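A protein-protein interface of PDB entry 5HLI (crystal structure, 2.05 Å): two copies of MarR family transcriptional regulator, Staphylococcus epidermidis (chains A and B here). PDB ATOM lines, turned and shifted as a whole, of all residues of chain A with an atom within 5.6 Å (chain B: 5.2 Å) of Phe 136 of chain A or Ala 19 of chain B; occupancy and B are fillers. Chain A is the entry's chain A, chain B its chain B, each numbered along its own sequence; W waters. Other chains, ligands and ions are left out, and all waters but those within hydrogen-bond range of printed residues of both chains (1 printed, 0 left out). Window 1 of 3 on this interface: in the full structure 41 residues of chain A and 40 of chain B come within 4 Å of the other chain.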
ATOM      1  N   ALA A  19       4.524  -4.121   4.926  1.00  0.00           N
ATOM      2  CA  ALA A  19       4.404  -4.221   3.475  1.00  0.00           C
ATOM      3  C   ALA A  19       5.291  -5.331   2.930  1.00  0.00           C
ATOM      4  O   ALA A  19       4.892  -6.066   2.019  1.00  0.00           O
ATOM      5  CB  ALA A  19       4.750  -2.882   2.823  1.00  0.00           C
ATOM      6  N   TYR A  20       6.502  -5.468   3.473  1.00  0.00           N
ATOM      7  CA  TYR A  20       7.377  -6.562   3.067  1.00  0.00           C
ATOM      8  C   TYR A  20       6.767  -7.907   3.433  1.00  0.00           C
ATOM      9  O   TYR A  20       6.744  -8.836   2.617  1.00  0.00           O
ATOM     10  CB  TYR A  20       8.752  -6.399   3.718  1.00  0.00           C
ATOM     11  CG  TYR A  20       9.789  -7.406   3.264  1.00  0.00           C
ATOM     12  CD1 TYR A  20       9.683  -8.043   2.035  1.00  0.00           C
ATOM     13  CD2 TYR A  20      10.875  -7.718   4.071  1.00  0.00           C
ATOM     14  CE1 TYR A  20      10.631  -8.956   1.620  1.00  0.00           C
ATOM     15  CE2 TYR A  20      11.828  -8.633   3.665  1.00  0.00           C
ATOM     16  CZ  TYR A  20      11.700  -9.250   2.439  1.00  0.00           C
ATOM     17  OH  TYR A  20      12.644 -10.162   2.027  1.00  0.00           O
ATOM     18  N   VAL A  22       3.690  -8.821   3.869  1.00  0.00           N
ATOM     19  CA  VAL A  22       2.566  -9.214   3.027  1.00  0.00           C
ATOM     20  C   VAL A  22       3.023  -9.473   1.593  1.00  0.00           C
ATOM     21  O   VAL A  22       2.471 -10.345   0.912  1.00  0.00           O
ATOM     22  CB  VAL A  22       1.437  -8.166   3.089  1.00  0.00           C
ATOM     23  CG1 VAL A  22       1.885  -6.839   2.522  1.00  0.00           C
ATOM     24  CG2 VAL A  22       0.201  -8.668   2.354  1.00  0.00           C
ATOM     25  N   SER A  23       4.041  -8.749   1.114  1.00  0.00           N
ATOM     26  CA  SER A  23       4.561  -9.023  -0.221  1.00  0.00           C
ATOM     27  C   SER A  23       5.166 -10.418  -0.303  1.00  0.00           C
ATOM     28  O   SER A  23       5.089 -11.065  -1.353  1.00  0.00           O
ATOM     29  CB  SER A  23       5.596  -7.968  -0.621  1.00  0.00           C
ATOM     30  OG  SER A  23       6.828  -8.175   0.048  1.00  0.00           O
ATOM     31  N   PHE A  26       2.242 -12.738  -0.923  1.00  0.00           N
ATOM     32  CA  PHE A  26       1.911 -12.717  -2.344  1.00  0.00           C
ATOM     33  C   PHE A  26       2.926 -13.515  -3.151  1.00  0.00           C
ATOM     34  O   PHE A  26       2.559 -14.245  -4.080  1.00  0.00           O
ATOM     35  CB  PHE A  26       1.841 -11.279  -2.853  1.00  0.00           C
ATOM     36  CG  PHE A  26       0.566 -10.567  -2.505  1.00  0.00           C
ATOM     37  CD1 PHE A  26      -0.638 -10.961  -3.064  1.00  0.00           C
ATOM     38  CD2 PHE A  26       0.574  -9.492  -1.633  1.00  0.00           C
ATOM     39  CE1 PHE A  26      -1.815 -10.304  -2.750  1.00  0.00           C
ATOM     40  CE2 PHE A  26      -0.596  -8.827  -1.318  1.00  0.00           C
ATOM     41  CZ  PHE A  26      -1.793  -9.234  -1.879  1.00  0.00           C
ATOM     42  N   GLU A 131      -5.731   2.041  -2.243  1.00  0.00           N
ATOM     43  CA  GLU A 131      -4.705   2.399  -1.267  1.00  0.00           C
ATOM     44  C   GLU A 131      -3.594   1.354  -1.229  1.00  0.00           C
ATOM     45  O   GLU A 131      -2.406   1.698  -1.199  1.00  0.00           O
ATOM     46  CB  GLU A 131      -5.332   2.580   0.118  1.00  0.00           C
ATOM     47  CG  GLU A 131      -4.377   2.323   1.282  1.00  0.00           C
ATOM     48  CD  GLU A 131      -4.855   2.940   2.582  1.00  0.00           C
ATOM     49  OE1 GLU A 131      -4.053   3.649   3.222  1.00  0.00           O
ATOM     50  OE2 GLU A 131      -6.022   2.706   2.951  1.00  0.00           O
ATOM     51  N   THR A 132      -3.963   0.072  -1.219  1.00  0.00           N
ATOM     52  CA  THR A 132      -2.961  -0.988  -1.256  1.00  0.00           C
ATOM     53  C   THR A 132      -2.176  -0.944  -2.560  1.00  0.00           C
ATOM     54  O   THR A 132      -0.944  -1.048  -2.562  1.00  0.00           O
ATOM     55  CB  THR A 132      -3.628  -2.353  -1.077  1.00  0.00           C
ATOM     56  OG1 THR A 132      -4.438  -2.341   0.105  1.00  0.00           O
ATOM     57  CG2 THR A 132      -2.578  -3.448  -0.957  1.00  0.00           C
ATOM     58  N   LYS A 133      -2.881  -0.793  -3.684  1.00  0.00           N
ATOM     59  CA  LYS A 133      -2.211  -0.607  -4.966  1.00  0.00           C
ATOM     60  C   LYS A 133      -1.274   0.595  -4.929  1.00  0.00           C
ATOM     61  O   LYS A 133      -0.145   0.527  -5.428  1.00  0.00           O
ATOM     62  CB  LYS A 133      -3.245  -0.441  -6.079  1.00  0.00           C
ATOM     63  CG  LYS A 133      -2.657  -0.130  -7.445  1.00  0.00           C
ATOM     64  CD  LYS A 133      -3.695   0.535  -8.338  1.00  0.00           C
ATOM     65  CE  LYS A 133      -3.157   0.776  -9.740  1.00  0.00           C
ATOM     66  NZ  LYS A 133      -2.865  -0.505 -10.435  1.00  0.00           N
ATOM     67  N   TYR A 134      -1.723   1.704  -4.333  1.00  0.00           N
ATOM     68  CA  TYR A 134      -0.916   2.921  -4.313  1.00  0.00           C
ATOM     69  C   TYR A 134       0.359   2.736  -3.499  1.00  0.00           C
ATOM     70  O   TYR A 134       1.425   3.226  -3.888  1.00  0.00           O
ATOM     71  CB  TYR A 134      -1.741   4.084  -3.759  1.00  0.00           C
ATOM     72  CG  TYR A 134      -0.962   5.365  -3.551  1.00  0.00           C
ATOM     73  CD1 TYR A 134      -0.350   6.010  -4.621  1.00  0.00           C
ATOM     74  CD2 TYR A 134      -0.845   5.931  -2.288  1.00  0.00           C
ATOM     75  CE1 TYR A 134       0.360   7.178  -4.437  1.00  0.00           C
ATOM     76  CE2 TYR A 134      -0.137   7.098  -2.092  1.00  0.00           C
ATOM     77  CZ  TYR A 134       0.463   7.717  -3.170  1.00  0.00           C
ATOM     78  OH  TYR A 134       1.169   8.882  -2.982  1.00  0.00           O
ATOM     79  N   VAL A 135       0.273   2.031  -2.370  1.00  0.00           N
ATOM     80  CA  VAL A 135       1.454   1.818  -1.535  1.00  0.00           C
ATOM     81  C   VAL A 135       2.481   0.967  -2.273  1.00  0.00           C
ATOM     82  O   VAL A 135       3.680   1.271  -2.277  1.00  0.00           O
ATOM     83  CB  VAL A 135       1.056   1.186  -0.190  1.00  0.00           C
ATOM     84  CG1 VAL A 135       2.291   0.744   0.574  1.00  0.00           C
ATOM     85  CG2 VAL A 135       0.246   2.173   0.636  1.00  0.00           C
ATOM     86  N   PHE A 136       2.025  -0.112  -2.916  1.00  0.00           N
ATOM     87  CA  PHE A 136       2.959  -0.998  -3.604  1.00  0.00           C
ATOM     88  C   PHE A 136       3.492  -0.378  -4.888  1.00  0.00           C
ATOM     89  O   PHE A 136       4.603  -0.710  -5.316  1.00  0.00           O
ATOM     90  CB  PHE A 136       2.295  -2.347  -3.887  1.00  0.00           C
ATOM     91  CG  PHE A 136       2.245  -3.255  -2.691  1.00  0.00           C
ATOM     92  CD1 PHE A 136       3.414  -3.762  -2.146  1.00  0.00           C
ATOM     93  CD2 PHE A 136       1.038  -3.596  -2.108  1.00  0.00           C
ATOM     94  CE1 PHE A 136       3.378  -4.594  -1.044  1.00  0.00           C
ATOM     95  CE2 PHE A 136       0.996  -4.430  -1.006  1.00  0.00           C
ATOM     96  CZ  PHE A 136       2.169  -4.930  -0.474  1.00  0.00           C
ATOM     97  N   GLU A 137       2.726   0.519  -5.517  1.00  0.00           N
ATOM     98  CA  GLU A 137       3.241   1.229  -6.684  1.00  0.00           C
ATOM     99  C   GLU A 137       4.381   2.163  -6.299  1.00  0.00           C
ATOM    100  O   GLU A 137       5.380   2.265  -7.022  1.00  0.00           O
ATOM    101  CB  GLU A 137       2.124   2.017  -7.370  1.00  0.00           C
ATOM    102  CG  GLU A 137       1.157   1.182  -8.191  1.00  0.00           C
ATOM    103  CD  GLU A 137       0.186   2.039  -8.982  1.00  0.00           C
ATOM    104  OE1 GLU A 137       0.413   2.234 -10.195  1.00  0.00           O
ATOM    105  OE2 GLU A 137      -0.796   2.532  -8.389  1.00  0.00           O
ATOM    106  N   GLU A 138       4.252   2.854  -5.165  1.00  0.00           N
ATOM    107  CA  GLU A 138       5.304   3.769  -4.740  1.00  0.00           C
ATOM    108  C   GLU A 138       6.511   3.029  -4.179  1.00  0.00           C
ATOM    109  O   GLU A 138       7.642   3.505  -4.322  1.00  0.00           O
ATOM    110  CB  GLU A 138       4.760   4.756  -3.707  1.00  0.00           C
ATOM    111  CG  GLU A 138       3.621   5.615  -4.230  1.00  0.00           C
ATOM    112  CD  GLU A 138       4.100   6.693  -5.185  1.00  0.00           C
ATOM    113  OE1 GLU A 138       3.413   6.936  -6.199  1.00  0.00           O
ATOM    114  OE2 GLU A 138       5.162   7.294  -4.923  1.00  0.00           O
ATOM    115  N   LEU A 139       6.298   1.870  -3.549  1.00  0.00           N
ATOM    116  CA  LEU A 139       7.430   1.057  -3.116  1.00  0.00           C
ATOM    117  C   LEU A 139       8.225   0.543  -4.309  1.00  0.00           C
ATOM    118  O   LEU A 139       9.460   0.512  -4.271  1.00  0.00           O
ATOM    119  CB  LEU A 139       6.945  -0.099  -2.242  1.00  0.00           C
ATOM    120  CG  LEU A 139       6.491   0.303  -0.836  1.00  0.00           C
ATOM    121  CD1 LEU A 139       5.863  -0.870  -0.112  1.00  0.00           C
ATOM    122  CD2 LEU A 139       7.662   0.861  -0.039  1.00  0.00           C
ATOM    123  N   GLU A 140       7.537   0.143  -5.384  1.00  0.00           N
ATOM    124  CA  GLU A 140       8.231  -0.259  -6.606  1.00  0.00           C
ATOM    125  C   GLU A 140       9.170   0.838  -7.093  1.00  0.00           C
ATOM    126  O   GLU A 140      10.319   0.572  -7.466  1.00  0.00           O
ATOM    127  CB  GLU A 140       7.221  -0.616  -7.700  1.00  0.00           C
ATOM    128  CG  GLU A 140       6.685  -2.039  -7.632  1.00  0.00           C
ATOM    129  CD  GLU A 140       5.981  -2.455  -8.913  1.00  0.00           C
ATOM    130  OE1 GLU A 140       4.755  -2.238  -9.026  1.00  0.00           O
ATOM    131  OE2 GLU A 140       6.660  -2.984  -9.817  1.00  0.00           O
ATOM    132  N   GLN A 141       8.684   2.075  -7.076  1.00  0.00           N
ATOM    133  CA  GLN A 141       9.460   3.214  -7.553  1.00  0.00           C
ATOM    134  C   GLN A 141      10.568   3.628  -6.585  1.00  0.00           C
ATOM    135  O   GLN A 141      11.688   3.919  -7.004  1.00  0.00           O
ATOM    136  CB  GLN A 141       8.541   4.405  -7.834  1.00  0.00           C
ATOM    137  CG  GLN A 141       7.932   4.404  -9.227  1.00  0.00           C
ATOM    138  CD  GLN A 141       7.373   5.758  -9.618  1.00  0.00           C
ATOM    139  OE1 GLN A 141       7.517   6.738  -8.886  1.00  0.00           O
ATOM    140  NE2 GLN A 141       6.730   5.820 -10.778  1.00  0.00           N
ATOM    141  N   LEU B  15      -2.381  -5.826  -9.033  1.00  0.00           N
ATOM    142  CA  LEU B  15      -1.977  -5.554  -7.685  1.00  0.00           C
ATOM    143  C   LEU B  15      -1.014  -6.603  -7.162  1.00  0.00           C
ATOM    144  O   LEU B  15      -0.017  -6.289  -6.584  1.00  0.00           O
ATOM    145  CB  LEU B  15      -3.186  -5.460  -6.767  1.00  0.00           C
ATOM    146  CG  LEU B  15      -2.818  -5.246  -5.317  1.00  0.00           C
ATOM    147  CD1 LEU B  15      -1.824  -4.158  -5.136  1.00  0.00           C
ATOM    148  CD2 LEU B  15      -4.029  -4.872  -4.540  1.00  0.00           C
ATOM    149  N   CYS B  16      -1.342  -7.853  -7.385  1.00  0.00           N
ATOM    150  CA  CYS B  16      -0.535  -8.928  -6.823  1.00  0.00           C
ATOM    151  C   CYS B  16       0.828  -9.023  -7.493  1.00  0.00           C
ATOM    152  O   CYS B  16       1.807  -9.405  -6.842  1.00  0.00           O
ATOM    153  CB  CYS B  16      -1.287 -10.248  -6.932  1.00  0.00           C
ATOM    154  SG  CYS B  16      -2.835 -10.239  -6.008  1.00  0.00           S
ATOM    155  N   PHE B  17       0.919  -8.676  -8.778  1.00  0.00           N
ATOM    156  CA  PHE B  17       2.217  -8.677  -9.443  1.00  0.00           C
ATOM    157  C   PHE B  17       3.079  -7.518  -8.957  1.00  0.00           C
ATOM    158  O   PHE B  17       4.302  -7.654  -8.837  1.00  0.00           O
ATOM    159  CB  PHE B  17       2.037  -8.616 -10.959  1.00  0.00           C
ATOM    160  CG  PHE B  17       3.264  -9.005 -11.730  1.00  0.00           C
ATOM    161  CD1 PHE B  17       3.665 -10.331 -11.794  1.00  0.00           C
ATOM    162  CD2 PHE B  17       4.018  -8.050 -12.390  1.00  0.00           C
ATOM    163  CE1 PHE B  17       4.795 -10.697 -12.500  1.00  0.00           C
ATOM    164  CE2 PHE B  17       5.151  -8.408 -13.100  1.00  0.00           C
ATOM    165  CZ  PHE B  17       5.540  -9.734 -13.156  1.00  0.00           C
ATOM    166  N   SER B  18       2.456  -6.373  -8.673  1.00  0.00           N
ATOM    167  CA  SER B  18       3.184  -5.257  -8.075  1.00  0.00           C
ATOM    168  C   SER B  18       3.800  -5.664  -6.742  1.00  0.00           C
ATOM    169  O   SER B  18       4.985  -5.418  -6.489  1.00  0.00           O
ATOM    170  CB  SER B  18       2.247  -4.061  -7.894  1.00  0.00           C
ATOM    171  OG  SER B  18       2.917  -2.969  -7.290  1.00  0.00           O
ATOM    172  N   ALA B  19       3.004  -6.298  -5.875  1.00  0.00           N
ATOM    173  CA  ALA B  19       3.524  -6.774  -4.597  1.00  0.00           C
ATOM    174  C   ALA B  19       4.576  -7.858  -4.798  1.00  0.00           C
ATOM    175  O   ALA B  19       5.554  -7.932  -4.046  1.00  0.00           O
ATOM    176  CB  ALA B  19       2.379  -7.294  -3.728  1.00  0.00           C
ATOM    177  N   TYR B  20       4.379  -8.717  -5.803  1.00  0.00           N
ATOM    178  CA  TYR B  20       5.383  -9.718  -6.157  1.00  0.00           C
ATOM    179  C   TYR B  20       6.728  -9.061  -6.457  1.00  0.00           C
ATOM    180  O   TYR B  20       7.773  -9.493  -5.954  1.00  0.00           O
ATOM    181  CB  TYR B  20       4.884 -10.519  -7.360  1.00  0.00           C
ATOM    182  CG  TYR B  20       5.549 -11.856  -7.603  1.00  0.00           C
ATOM    183  CD1 TYR B  20       6.281 -12.497  -6.611  1.00  0.00           C
ATOM    184  CD2 TYR B  20       5.442 -12.477  -8.841  1.00  0.00           C
ATOM    185  CE1 TYR B  20       6.880 -13.735  -6.853  1.00  0.00           C
ATOM    186  CE2 TYR B  20       6.033 -13.695  -9.090  1.00  0.00           C
ATOM    187  CZ  TYR B  20       6.750 -14.322  -8.099  1.00  0.00           C
ATOM    188  OH  TYR B  20       7.329 -15.540  -8.376  1.00  0.00           O
ATOM    189  N   ASN B  21       6.717  -8.008  -7.281  1.00  0.00           N
ATOM    190  CA  ASN B  21       7.943  -7.261  -7.551  1.00  0.00           C
ATOM    191  C   ASN B  21       8.526  -6.677  -6.271  1.00  0.00           C
ATOM    192  O   ASN B  21       9.741  -6.730  -6.050  1.00  0.00           O
ATOM    193  CB  ASN B  21       7.671  -6.146  -8.562  1.00  0.00           C
ATOM    194  CG  ASN B  21       7.513  -6.662  -9.979  1.00  0.00           C
ATOM    195  OD1 ASN B  21       7.991  -7.744 -10.318  1.00  0.00           O
ATOM    196  ND2 ASN B  21       6.838  -5.883 -10.817  1.00  0.00           N
ATOM    197  N   VAL B  22       7.669  -6.120  -5.413  1.00  0.00           N
ATOM    198  CA  VAL B  22       8.134  -5.482  -4.184  1.00  0.00           C
ATOM    199  C   VAL B  22       8.838  -6.484  -3.278  1.00  0.00           C
ATOM    200  O   VAL B  22       9.812  -6.135  -2.599  1.00  0.00           O
ATOM    201  CB  VAL B  22       6.949  -4.791  -3.477  1.00  0.00           C
ATOM    202  CG1 VAL B  22       7.286  -4.463  -2.036  1.00  0.00           C
ATOM    203  CG2 VAL B  22       6.562  -3.525  -4.225  1.00  0.00           C
ATOM    204  N   SER B  23       8.381  -7.741  -3.264  1.00  0.00           N
ATOM    205  CA  SER B  23       9.042  -8.755  -2.447  1.00  0.00           C
ATOM    206  C   SER B  23      10.503  -8.922  -2.846  1.00  0.00           C
ATOM    207  O   SER B  23      11.373  -9.106  -1.987  1.00  0.00           O
ATOM    208  CB  SER B  23       8.303 -10.092  -2.552  1.00  0.00           C
ATOM    209  OG  SER B  23       8.452 -10.672  -3.839  1.00  0.00           O
HETATM  210  O   HOH W   1       4.251  -4.093 -11.395  1.00  0.00           O
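Ser 23 of chain A touches Ala 19 of chain B.
OG of Ser 23 of chain A touches CA of Ser 23 of chain B (3.4 Å).
SG of Cys 16 of chain B touches CE1 of Phe 26 of chain A, 3.4 Å away.
CD2 of Phe 26 of chain A touches CB of Ala 19 of chain B, at 3.5 Å.
Leu 15 of chain B touches Lys 133 of chain A (CD1 to CA, 3.6 Å).
Phe 136 of chain A touches Ala 19 of chain B.
Phe 136 of chain A touches Val 22 of chain B.
OG of Ser 18 of chain B touches N of Glu 137 of chain A, at 3.9 Å.
Val 22 of chain B touches Leu 139 of chain A (CG2 to CB, 3.98 Å).
CG of Glu 140 of chain A touches CG2 of Val 22 of chain B, 3.7 Å away.
Tyr 20 of chain A touches Ser 23 of chain B, but with the chains exchanged Ser 23 of chain A does not touch Tyr 20 of chain B (5.0 Å).
Ser 23 of chain A touches Ala 19 of chain B, but with the chains exchanged Ala 19 of chain A does not touch Ser 23 of chain B (6.5 Å).
Ser 23 of chain A touches its own counterpart, Ser 23 of chain B.
Phe 136 of chain A touches just these residues of chain B: Ser 18, Ala 19 and Val 22.
Printed residues of chain B within 4 Å of Lys 133 of chain A: Leu 15 (3.6 Å).
Of the printed residues of chain B, Phe 26 of chain A touches Cys 16 (3.4 Å) and Ala 19 (3.5 Å).
Printed residues of chain B within 4 Å of Glu 137 of chain A: Ser 18 (3.9 Å).
The nearest residue of chain B that does not touch Phe 136 of chain A is Leu 15 of chain B (4.2 Å).
The nearest residue of chain A that does not touch Ala 19 of chain B is Glu 140 of chain A (5.4 Å).
The side-chain hydroxyl (OG) of Ser 23 of chain A lies close to the backbone carbonyl oxygen (O) of Ala 19 of chain A (3.5 Å).
The side-chain hydroxyl (OG) of Ser 23 of chain A lies within hydrogen-bond range of the backbone carbonyl oxygen (O) of Tyr 20 of chain A (2.7 Å).
The side-chain hydroxyl (OG) of Ser 23 of chain B lies within hydrogen-bond range of the backbone carbonyl oxygen (O) of Tyr 20 of chain B (2.5 Å).
Printed residues of chain B that touch a printed residue of chain A: Leu 15, Cys 16, Ser 18, Ala 19, Asn 21, Val 22 and Ser 23.
Hydrophobic or aromatic side chains of chain B within 4 Å of the printed part of chain A: Leu 15, Ala 19 and Val 22.
Of the 16 printed residues of chain A, 8 touch a printed residue of chain B.
Hydrophobic or aromatic side chains of chain A within 4 Å of the printed part of chain B: Tyr 20, Phe 26, Phe 136 and Leu 139.
Among the printed residues, 14 pairs touch across the chains.
Among the printed residues, no Asp or Glu carboxylate lies within 4 Å of a Lys or Arg side-chain nitrogen of the other chain.
Water W1 bridges the side-chain carboxylate (OE1) of Glu 140 of chain A (3.1 Å) and the side-chain amide nitrogen (ND2) of Asn 21 of chain B (3.2 Å).
The side-chain hydroxyl of Ser 18 of chain B sits at hydrogen-bond distance from the backbone carbonyl oxygen of Phe 136 of chain A, at 3.4 Å.
OG of Ser 18 of chain B sits at hydrogen-bond distance from OE1 of Glu 140 of chain A.
The side-chain amide nitrogen (ND2) of Asn 21 of chain B lies within hydrogen-bond range of the side-chain carboxylate (OE2) of Glu 140 of chain A, at 3.1 Å.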
